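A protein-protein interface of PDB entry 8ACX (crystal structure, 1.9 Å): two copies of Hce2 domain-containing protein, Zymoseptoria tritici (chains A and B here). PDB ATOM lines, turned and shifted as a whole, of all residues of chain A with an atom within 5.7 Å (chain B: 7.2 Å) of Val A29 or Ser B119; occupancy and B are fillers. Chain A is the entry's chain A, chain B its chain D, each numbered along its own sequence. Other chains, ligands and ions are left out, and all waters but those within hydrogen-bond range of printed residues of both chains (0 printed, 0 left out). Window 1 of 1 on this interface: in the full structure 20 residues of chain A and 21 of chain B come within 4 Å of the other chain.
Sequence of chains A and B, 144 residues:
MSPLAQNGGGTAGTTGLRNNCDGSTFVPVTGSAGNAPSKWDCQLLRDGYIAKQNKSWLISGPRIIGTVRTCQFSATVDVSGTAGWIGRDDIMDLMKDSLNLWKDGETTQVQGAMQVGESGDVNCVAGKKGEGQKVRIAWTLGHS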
ATOM      1  N   VAL A  27      14.047 -18.262 -12.830  1.00  0.00           N
ATOM      2  CA  VAL A  27      13.534 -17.793 -14.147  1.00  0.00           C
ATOM      3  C   VAL A  27      13.207 -16.314 -14.010  1.00  0.00           C
ATOM      4  O   VAL A  27      12.336 -15.941 -13.223  1.00  0.00           O
ATOM      5  CB  VAL A  27      12.311 -18.628 -14.541  1.00  0.00           C
ATOM      6  CG1 VAL A  27      11.711 -18.176 -15.855  1.00  0.00           C
ATOM      7  CG2 VAL A  27      12.665 -20.109 -14.585  1.00  0.00           C
ATOM      8  N   PRO A  28      13.872 -15.416 -14.768  1.00  0.00           N
ATOM      9  CA  PRO A  28      13.501 -14.009 -14.753  1.00  0.00           C
ATOM     10  C   PRO A  28      12.149 -13.856 -15.472  1.00  0.00           C
ATOM     11  O   PRO A  28      11.954 -14.371 -16.546  1.00  0.00           O
ATOM     12  CB  PRO A  28      14.695 -13.308 -15.434  1.00  0.00           C
ATOM     13  CG  PRO A  28      15.268 -14.350 -16.355  1.00  0.00           C
ATOM     14  CD  PRO A  28      14.993 -15.685 -15.672  1.00  0.00           C
ATOM     15  N   VAL A  29      11.218 -13.210 -14.793  1.00  0.00           N
ATOM     16  CA  VAL A  29       9.837 -12.963 -15.294  1.00  0.00           C
ATOM     17  C   VAL A  29       9.830 -11.594 -15.984  1.00  0.00           C
ATOM     18  O   VAL A  29      10.232 -10.611 -15.379  1.00  0.00           O
ATOM     19  CB  VAL A  29       8.808 -13.088 -14.148  1.00  0.00           C
ATOM     20  CG1 VAL A  29       7.397 -12.760 -14.577  1.00  0.00           C
ATOM     21  CG2 VAL A  29       8.879 -14.476 -13.543  1.00  0.00           C
ATOM     22  N   THR A  30       9.409 -11.569 -17.241  1.00  0.00           N
ATOM     23  CA  THR A  30       9.328 -10.355 -18.075  1.00  0.00           C
ATOM     24  C   THR A  30       7.878  -9.850 -18.049  1.00  0.00           C
ATOM     25  O   THR A  30       6.938 -10.647 -17.879  1.00  0.00           O
ATOM     26  CB  THR A  30       9.879 -10.611 -19.479  1.00  0.00           C
ATOM     27  OG1 THR A  30      11.272 -10.896 -19.407  1.00  0.00           O
ATOM     28  CG2 THR A  30       9.831  -9.380 -20.368  1.00  0.00           C
ATOM     29  N   GLY A  31       7.714  -8.546 -18.207  1.00  0.00           N
ATOM     30  CA  GLY A  31       6.411  -7.877 -18.258  1.00  0.00           C
ATOM     31  C   GLY A  31       6.533  -6.455 -18.741  1.00  0.00           C
ATOM     32  O   GLY A  31       7.645  -6.042 -19.056  1.00  0.00           O
ATOM     33  N   MET A 114      10.111  -5.034 -19.261  1.00  0.00           N
ATOM     34  CA  MET A 114      11.100  -4.898 -18.161  1.00  0.00           C
ATOM     35  C   MET A 114      11.024  -6.135 -17.264  1.00  0.00           C
ATOM     36  O   MET A 114       9.936  -6.742 -17.196  1.00  0.00           O
ATOM     37  CB  MET A 114      10.777  -3.665 -17.313  1.00  0.00           C
ATOM     38  CG  MET A 114       9.391  -3.724 -16.700  1.00  0.00           C
ATOM     39  SD  MET A 114       9.183  -2.605 -15.294  1.00  0.00           S
ATOM     40  CE  MET A 114      10.896  -2.244 -14.914  1.00  0.00           C
ATOM     41  N   GLN A 115      12.131  -6.508 -16.613  1.00  0.00           N
ATOM     42  CA  GLN A 115      12.025  -7.627 -15.640  1.00  0.00           C
ATOM     43  C   GLN A 115      11.062  -7.163 -14.546  1.00  0.00           C
ATOM     44  O   GLN A 115      11.254  -6.046 -14.029  1.00  0.00           O
ATOM     45  CB  GLN A 115      13.374  -8.043 -15.049  1.00  0.00           C
ATOM     46  CG  GLN A 115      13.249  -9.251 -14.129  1.00  0.00           C
ATOM     47  CD  GLN A 115      14.558  -9.699 -13.529  1.00  0.00           C
ATOM     48  OE1 GLN A 115      15.635  -9.360 -14.013  1.00  0.00           O
ATOM     49  NE2 GLN A 115      14.471 -10.473 -12.460  1.00  0.00           N
ATOM     50  N   VAL A 116      10.057  -7.976 -14.229  1.00  0.00           N
ATOM     51  CA  VAL A 116       9.018  -7.571 -13.244  1.00  0.00           C
ATOM     52  C   VAL A 116       9.021  -8.543 -12.075  1.00  0.00           C
ATOM     53  O   VAL A 116       8.252  -8.299 -11.105  1.00  0.00           O
ATOM     54  CB  VAL A 116       7.625  -7.469 -13.893  1.00  0.00           C
ATOM     55  CG1 VAL A 116       7.605  -6.346 -14.931  1.00  0.00           C
ATOM     56  CG2 VAL A 116       7.184  -8.787 -14.473  1.00  0.00           C
ATOM     57  N   GLY A 117       9.863  -9.577 -12.135  1.00  0.00           N
ATOM     58  CA  GLY A 117       9.861 -10.632 -11.106  1.00  0.00           C
ATOM     59  C   GLY A 117      10.892 -11.726 -11.332  1.00  0.00           C
ATOM     60  O   GLY A 117      11.696 -11.659 -12.312  1.00  0.00           O
ATOM     61  N   GLU A 118      10.933 -12.640 -10.342  1.00  0.00           N
ATOM     62  CA  GLU A 118      11.680 -13.921 -10.442  1.00  0.00           C
ATOM     63  C   GLU A 118      10.743 -15.028  -9.987  1.00  0.00           C
ATOM     64  O   GLU A 118      10.023 -14.847  -8.981  1.00  0.00           O
ATOM     65  CB  GLU A 118      12.968 -13.897  -9.620  1.00  0.00           C
ATOM     66  CG  GLU A 118      13.989 -14.957  -9.994  1.00  0.00           C
ATOM     67  CD  GLU A 118      14.932 -14.591 -11.151  1.00  0.00           C
ATOM     68  OE1 GLU A 118      14.938 -13.415 -11.595  1.00  0.00           O
ATOM     69  OE2 GLU A 118      15.632 -15.518 -11.654  1.00  0.00           O
ATOM     70  N   SER A 119      10.742 -16.128 -10.730  1.00  0.00           N
ATOM     71  CA  SER A 119      10.078 -17.386 -10.358  1.00  0.00           C
ATOM     72  C   SER A 119      11.084 -18.522 -10.343  1.00  0.00           C
ATOM     73  O   SER A 119      12.214 -18.372 -10.880  1.00  0.00           O
ATOM     74  CB  SER A 119       8.950 -17.655 -11.293  1.00  0.00           C
ATOM     75  OG  SER A 119       7.905 -16.694 -11.064  1.00  0.00           O
ATOM     76  N   SER B  24      11.836 -26.701 -23.026  1.00  0.00           N
ATOM     77  CA  SER B  24      11.579 -25.510 -22.177  1.00  0.00           C
ATOM     78  C   SER B  24      10.933 -25.888 -20.841  1.00  0.00           C
ATOM     79  O   SER B  24       9.905 -26.580 -20.870  1.00  0.00           O
ATOM     80  CB  SER B  24      10.712 -24.515 -22.902  1.00  0.00           C
ATOM     81  OG  SER B  24       9.832 -23.860 -22.001  1.00  0.00           O
ATOM     82  N   THR B  25      11.530 -25.484 -19.717  1.00  0.00           N
ATOM     83  CA  THR B  25      10.893 -25.651 -18.388  1.00  0.00           C
ATOM     84  C   THR B  25       9.568 -24.881 -18.384  1.00  0.00           C
ATOM     85  O   THR B  25       9.346 -24.022 -19.266  1.00  0.00           O
ATOM     86  CB  THR B  25      11.856 -25.241 -17.271  1.00  0.00           C
ATOM     87  OG1 THR B  25      12.140 -23.850 -17.405  1.00  0.00           O
ATOM     88  CG2 THR B  25      13.147 -26.036 -17.307  1.00  0.00           C
ATOM     89  N   PHE B  26       8.697 -25.217 -17.452  1.00  0.00           N
ATOM     90  CA  PHE B  26       7.371 -24.596 -17.245  1.00  0.00           C
ATOM     91  C   PHE B  26       7.199 -24.347 -15.751  1.00  0.00           C
ATOM     92  O   PHE B  26       7.156 -25.296 -14.992  1.00  0.00           O
ATOM     93  CB  PHE B  26       6.240 -25.469 -17.791  1.00  0.00           C
ATOM     94  CG  PHE B  26       6.275 -25.591 -19.286  1.00  0.00           C
ATOM     95  CD1 PHE B  26       7.033 -26.582 -19.900  1.00  0.00           C
ATOM     96  CD2 PHE B  26       5.636 -24.652 -20.071  1.00  0.00           C
ATOM     97  CE1 PHE B  26       7.094 -26.659 -21.279  1.00  0.00           C
ATOM     98  CE2 PHE B  26       5.711 -24.720 -21.448  1.00  0.00           C
ATOM     99  CZ  PHE B  26       6.422 -25.730 -22.047  1.00  0.00           C
ATOM    100  N   VAL B  27       7.127 -23.079 -15.362  1.00  0.00           N
ATOM    101  CA  VAL B  27       6.962 -22.636 -13.950  1.00  0.00           C
ATOM    102  C   VAL B  27       5.658 -21.851 -13.867  1.00  0.00           C
ATOM    103  O   VAL B  27       5.525 -20.814 -14.505  1.00  0.00           O
ATOM    104  CB  VAL B  27       8.179 -21.797 -13.531  1.00  0.00           C
ATOM    105  CG1 VAL B  27       8.062 -21.292 -12.120  1.00  0.00           C
ATOM    106  CG2 VAL B  27       9.473 -22.578 -13.719  1.00  0.00           C
ATOM    107  N   PRO B  28       4.662 -22.293 -13.070  1.00  0.00           N
ATOM    108  CA  PRO B  28       3.446 -21.508 -12.882  1.00  0.00           C
ATOM    109  C   PRO B  28       3.792 -20.282 -12.023  1.00  0.00           C
ATOM    110  O   PRO B  28       4.431 -20.398 -11.012  1.00  0.00           O
ATOM    111  CB  PRO B  28       2.454 -22.517 -12.253  1.00  0.00           C
ATOM    112  CG  PRO B  28       3.335 -23.494 -11.530  1.00  0.00           C
ATOM    113  CD  PRO B  28       4.630 -23.554 -12.328  1.00  0.00           C
ATOM    114  N   VAL B  29       3.413 -19.115 -12.516  1.00  0.00           N
ATOM    115  CA  VAL B  29       3.660 -17.801 -11.850  1.00  0.00           C
ATOM    116  C   VAL B  29       2.434 -17.467 -11.001  1.00  0.00           C
ATOM    117  O   VAL B  29       1.339 -17.472 -11.518  1.00  0.00           O
ATOM    118  CB  VAL B  29       4.014 -16.713 -12.878  1.00  0.00           C
ATOM    119  CG1 VAL B  29       4.199 -15.329 -12.241  1.00  0.00           C
ATOM    120  CG2 VAL B  29       5.247 -17.118 -13.674  1.00  0.00           C
ATOM    121  N   SER B  74       6.259 -12.391 -23.636  1.00  0.00           N
ATOM    122  CA  SER B  74       7.531 -11.626 -23.558  1.00  0.00           C
ATOM    123  C   SER B  74       8.712 -12.547 -23.215  1.00  0.00           C
ATOM    124  O   SER B  74       8.478 -13.743 -22.856  1.00  0.00           O
ATOM    125  CB  SER B  74       7.424 -10.472 -22.608  1.00  0.00           C
ATOM    126  OG  SER B  74       7.141 -10.943 -21.307  1.00  0.00           O
ATOM    127  N   THR B  76      13.394 -12.600 -22.345  1.00  0.00           N
ATOM    128  CA  THR B  76      14.713 -12.010 -22.083  1.00  0.00           C
ATOM    129  C   THR B  76      15.760 -13.123 -22.206  1.00  0.00           C
ATOM    130  O   THR B  76      15.419 -14.280 -22.373  1.00  0.00           O
ATOM    131  CB  THR B  76      14.705 -11.292 -20.727  1.00  0.00           C
ATOM    132  OG1 THR B  76      15.845 -10.462 -20.794  1.00  0.00           O
ATOM    133  CG2 THR B  76      14.769 -12.178 -19.512  1.00  0.00           C
ATOM    134  N   SER B  98       1.384 -24.002 -21.979  1.00  0.00           N
ATOM    135  CA  SER B  98       1.165 -23.159 -20.773  1.00  0.00           C
ATOM    136  C   SER B  98      -0.339 -23.112 -20.450  1.00  0.00           C
ATOM    137  O   SER B  98      -0.696 -23.209 -19.299  1.00  0.00           O
ATOM    138  CB  SER B  98       1.736 -21.766 -20.978  1.00  0.00           C
ATOM    139  OG  SER B  98       3.150 -21.802 -21.189  1.00  0.00           O
ATOM    140  N   GLN B 115      -2.968 -18.408 -10.076  1.00  0.00           N
ATOM    141  CA  GLN B 115      -1.955 -18.415 -11.155  1.00  0.00           C
ATOM    142  C   GLN B 115      -2.221 -17.198 -12.057  1.00  0.00           C
ATOM    143  O   GLN B 115      -3.366 -16.979 -12.481  1.00  0.00           O
ATOM    144  CB  GLN B 115      -1.950 -19.759 -11.878  1.00  0.00           C
ATOM    145  CG  GLN B 115      -0.825 -19.846 -12.892  1.00  0.00           C
ATOM    146  CD  GLN B 115      -0.738 -21.175 -13.583  1.00  0.00           C
ATOM    147  OE1 GLN B 115      -1.400 -22.126 -13.199  1.00  0.00           O
ATOM    148  NE2 GLN B 115       0.081 -21.240 -14.618  1.00  0.00           N
ATOM    149  N   GLY B 117       0.183 -16.386 -14.540  1.00  0.00           N
ATOM    150  CA  GLY B 117       1.097 -16.573 -15.669  1.00  0.00           C
ATOM    151  C   GLY B 117       1.816 -17.905 -15.682  1.00  0.00           C
ATOM    152  O   GLY B 117       1.583 -18.764 -14.811  1.00  0.00           O
ATOM    153  N   GLU B 118       2.593 -18.097 -16.748  1.00  0.00           N
ATOM    154  CA  GLU B 118       3.574 -19.202 -16.898  1.00  0.00           C
ATOM    155  C   GLU B 118       4.880 -18.579 -17.400  1.00  0.00           C
ATOM    156  O   GLU B 118       4.837 -17.726 -18.296  1.00  0.00           O
ATOM    157  CB  GLU B 118       3.066 -20.291 -17.861  1.00  0.00           C
ATOM    158  CG  GLU B 118       3.764 -21.627 -17.713  1.00  0.00           C
ATOM    159  CD  GLU B 118       3.227 -22.565 -16.632  1.00  0.00           C
ATOM    160  OE1 GLU B 118       2.160 -22.278 -16.061  1.00  0.00           O
ATOM    161  OE2 GLU B 118       3.916 -23.578 -16.335  1.00  0.00           O
ATOM    162  N   SER B 119       5.987 -19.010 -16.823  1.00  0.00           N
ATOM    163  CA  SER B 119       7.347 -18.733 -17.302  1.00  0.00           C
ATOM    164  C   SER B 119       8.089 -20.044 -17.565  1.00  0.00           C
ATOM    165  O   SER B 119       7.656 -21.111 -17.105  1.00  0.00           O
ATOM    166  CB  SER B 119       8.050 -17.883 -16.304  1.00  0.00           C
ATOM    167  OG  SER B 119       7.477 -16.563 -16.304  1.00  0.00           O
ATOM    168  N   GLY B 120       9.209 -19.904 -18.261  1.00  0.00           N
ATOM    169  CA  GLY B 120      10.056 -21.027 -18.683  1.00  0.00           C
ATOM    170  C   GLY B 120      11.406 -20.567 -19.164  1.00  0.00           C
ATOM    171  O   GLY B 120      11.597 -19.369 -19.529  1.00  0.00           O
ATOM    172  N   ASP B 121      12.327 -21.508 -19.134  1.00  0.00           N
ATOM    173  CA  ASP B 121      13.697 -21.343 -19.652  1.00  0.00           C
ATOM    174  C   ASP B 121      13.891 -22.368 -20.777  1.00  0.00           C
ATOM    175  O   ASP B 121      13.593 -23.582 -20.581  1.00  0.00           O
ATOM    176  CB  ASP B 121      14.690 -21.458 -18.506  1.00  0.00           C
ATOM    177  CG  ASP B 121      15.861 -20.549 -18.758  1.00  0.00           C
ATOM    178  OD1 ASP B 121      15.612 -19.381 -19.121  1.00  0.00           O
ATOM    179  OD2 ASP B 121      16.992 -21.019 -18.688  1.00  0.00           O
ATOM    180  N   ALA B 138      14.626 -16.898 -21.318  1.00  0.00           N
ATOM    181  CA  ALA B 138      13.584 -16.899 -20.273  1.00  0.00           C
ATOM    182  C   ALA B 138      12.349 -16.225 -20.866  1.00  0.00           C
ATOM    183  O   ALA B 138      12.410 -14.987 -21.098  1.00  0.00           O
ATOM    184  CB  ALA B 138      14.062 -16.147 -19.046  1.00  0.00           C
ATOM    185  N   TRP B 139      11.282 -16.986 -21.079  1.00  0.00           N
ATOM    186  CA  TRP B 139       9.995 -16.474 -21.613  1.00  0.00           C
ATOM    187  C   TRP B 139       8.960 -16.357 -20.485  1.00  0.00           C
ATOM    188  O   TRP B 139       9.163 -16.967 -19.408  1.00  0.00           O
ATOM    189  CB  TRP B 139       9.513 -17.346 -22.779  1.00  0.00           C
ATOM    190  CG  TRP B 139       9.235 -18.761 -22.373  1.00  0.00           C
ATOM    191  CD1 TRP B 139      10.124 -19.785 -22.397  1.00  0.00           C
ATOM    192  CD2 TRP B 139       8.011 -19.293 -21.831  1.00  0.00           C
ATOM    193  NE1 TRP B 139       9.543 -20.928 -21.906  1.00  0.00           N
ATOM    194  CE2 TRP B 139       8.250 -20.662 -21.548  1.00  0.00           C
ATOM    195  CE3 TRP B 139       6.744 -18.752 -21.528  1.00  0.00           C
ATOM    196  CZ2 TRP B 139       7.278 -21.499 -21.008  1.00  0.00           C
ATOM    197  CZ3 TRP B 139       5.801 -19.572 -20.954  1.00  0.00           C
ATOM    198  CH2 TRP B 139       6.056 -20.921 -20.715  1.00  0.00           C
ATOM    199  N   THR B 140       7.951 -15.516 -20.713  1.00  0.00           N
ATOM    200  CA  THR B 140       6.793 -15.241 -19.845  1.00  0.00           C
ATOM    201  C   THR B 140       5.525 -15.102 -20.694  1.00  0.00           C
ATOM    202  O   THR B 140       5.475 -14.300 -21.665  1.00  0.00           O
ATOM    203  CB  THR B 140       7.007 -13.979 -18.991  1.00  0.00           C
ATOM    204  OG1 THR B 140       8.159 -14.197 -18.153  1.00  0.00           O
ATOM    205  CG2 THR B 140       5.773 -13.625 -18.175  1.00  0.00           C
ATOM    206  N   LEU B 141       4.510 -15.859 -20.306  1.00  0.00           N
ATOM    207  CA  LEU B 141       3.099 -15.632 -20.695  1.00  0.00           C
ATOM    208  C   LEU B 141       2.371 -15.036 -19.492  1.00  0.00           C
ATOM    209  O   LEU B 141       2.375 -15.648 -18.446  1.00  0.00           O
ATOM    210  CB  LEU B 141       2.503 -16.957 -21.148  1.00  0.00           C
ATOM    211  CG  LEU B 141       1.004 -16.958 -21.404  1.00  0.00           C
ATOM    212  CD1 LEU B 141       0.658 -16.026 -22.560  1.00  0.00           C
ATOM    213  CD2 LEU B 141       0.529 -18.368 -21.749  1.00  0.00           C
ATOM    214  N   GLY B 142       1.820 -13.840 -19.611  1.00  0.00           N
ATOM    215  CA  GLY B 142       1.169 -13.185 -18.462  1.00  0.00           C
ATOM    216  C   GLY B 142       0.360 -11.953 -18.814  1.00  0.00           C
ATOM    217  O   GLY B 142       0.133 -11.722 -19.991  1.00  0.00           O
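Hydrophobic or aromatic side chains of chain B within 4 Å of the printed part of chain A: Val B27, Val B29 and Ala B138. Of the 11 printed residues of chain A, 6 touch a printed residue of chain B. Printed residues of chain A that touch a printed residue of chain B: Val A27, Pro A28, Val A29, Thr A30, Gly A31 and Ser A119.
Printed residues of chain B within 4 Å of Pro A28: Thr B76 and Ala B138. Of chain B, only Ser B119 and Thr B140 come within 4 Å of Val A29. Gly A117 touches none of the printed residues of chain B. Of the printed residues of chain B, Ser A119 touches Val B27 (3.8 Å) and Val B29 (3.7 Å). Ser B24 touches none of the printed residues of chain A. Printed residues of chain A within 4 Å of Thr B76: Pro A28 (3.9 Å) and Thr A30 (3.7 Å). Ser B119 touches two residues of chain A. Printed residues of chain A within 4 Å of Thr B140: Val A29 and Thr A30. The nearest residue of chain A that does not touch Ser B119 is Pro A28 (5.0 Å).
The side-chain hydroxyl (OG1) of Thr B140 sits at hydrogen-bond distance from the backbone NH (N) of Thr A30 (3.0 Å). The backbone carbonyl oxygen (O) of Thr A30 sits close to the side-chain hydroxyl (OG) of Ser B74, at 3.4 Å.
OE2 of Glu A118 sits at hydrogen-bond distance from N of Val A27, at 3.4 Å. O of Val A29 is in hydrogen-bond range of N of Val A116. The backbone NH (N) of Val B29 is in hydrogen-bond range of the backbone carbonyl oxygen (O) of Gly B117 (3.0 Å). The backbone carbonyl oxygen of Gly B120 lies within hydrogen-bond range of the backbone NH of Trp B139 (2.9 Å). The backbone carbonyl oxygen (O) of Ser B74 is in hydrogen-bond range of the backbone NH (N) of Thr B140 (2.8 Å). OE2 of Glu B118 is in hydrogen-bond range of N of Val B27 (3.4 Å).
Val A27 touches Ser B119, and with the chains exchanged Ser A119 touches Val B27. Val A29 touches Ser B119, and with the chains exchanged Ser A119 touches Val B29. 7 positions are printed for both chains. Of the 12 pairs that touch across the chains among the printed residues, 4 have their exchanged pair printed and touching as well.
CG1 of Val A27 touches CB of Ser B119, at 3.7 Å. Val A27 touches Gly B120. Thr B76 touches Pro A28 (CG2 to CG, 3.9 Å). CB of Ala B138 touches CG of Pro A28, at 3.5 Å. Ser B119 touches Val A29 (OG to CG2, 3.7 Å). Thr B140 touches Val A29 (OG1 to CA, 3.5 Å). Thr B76 touches Thr A30. OG of Ser B74 touches N of Gly A31, at 3.96 Å. CB of Ser A119 touches CG1 of Val B27, 3.8 Å away. Val B29 touches Ser A119 (CG2 to OG, 3.7 Å).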
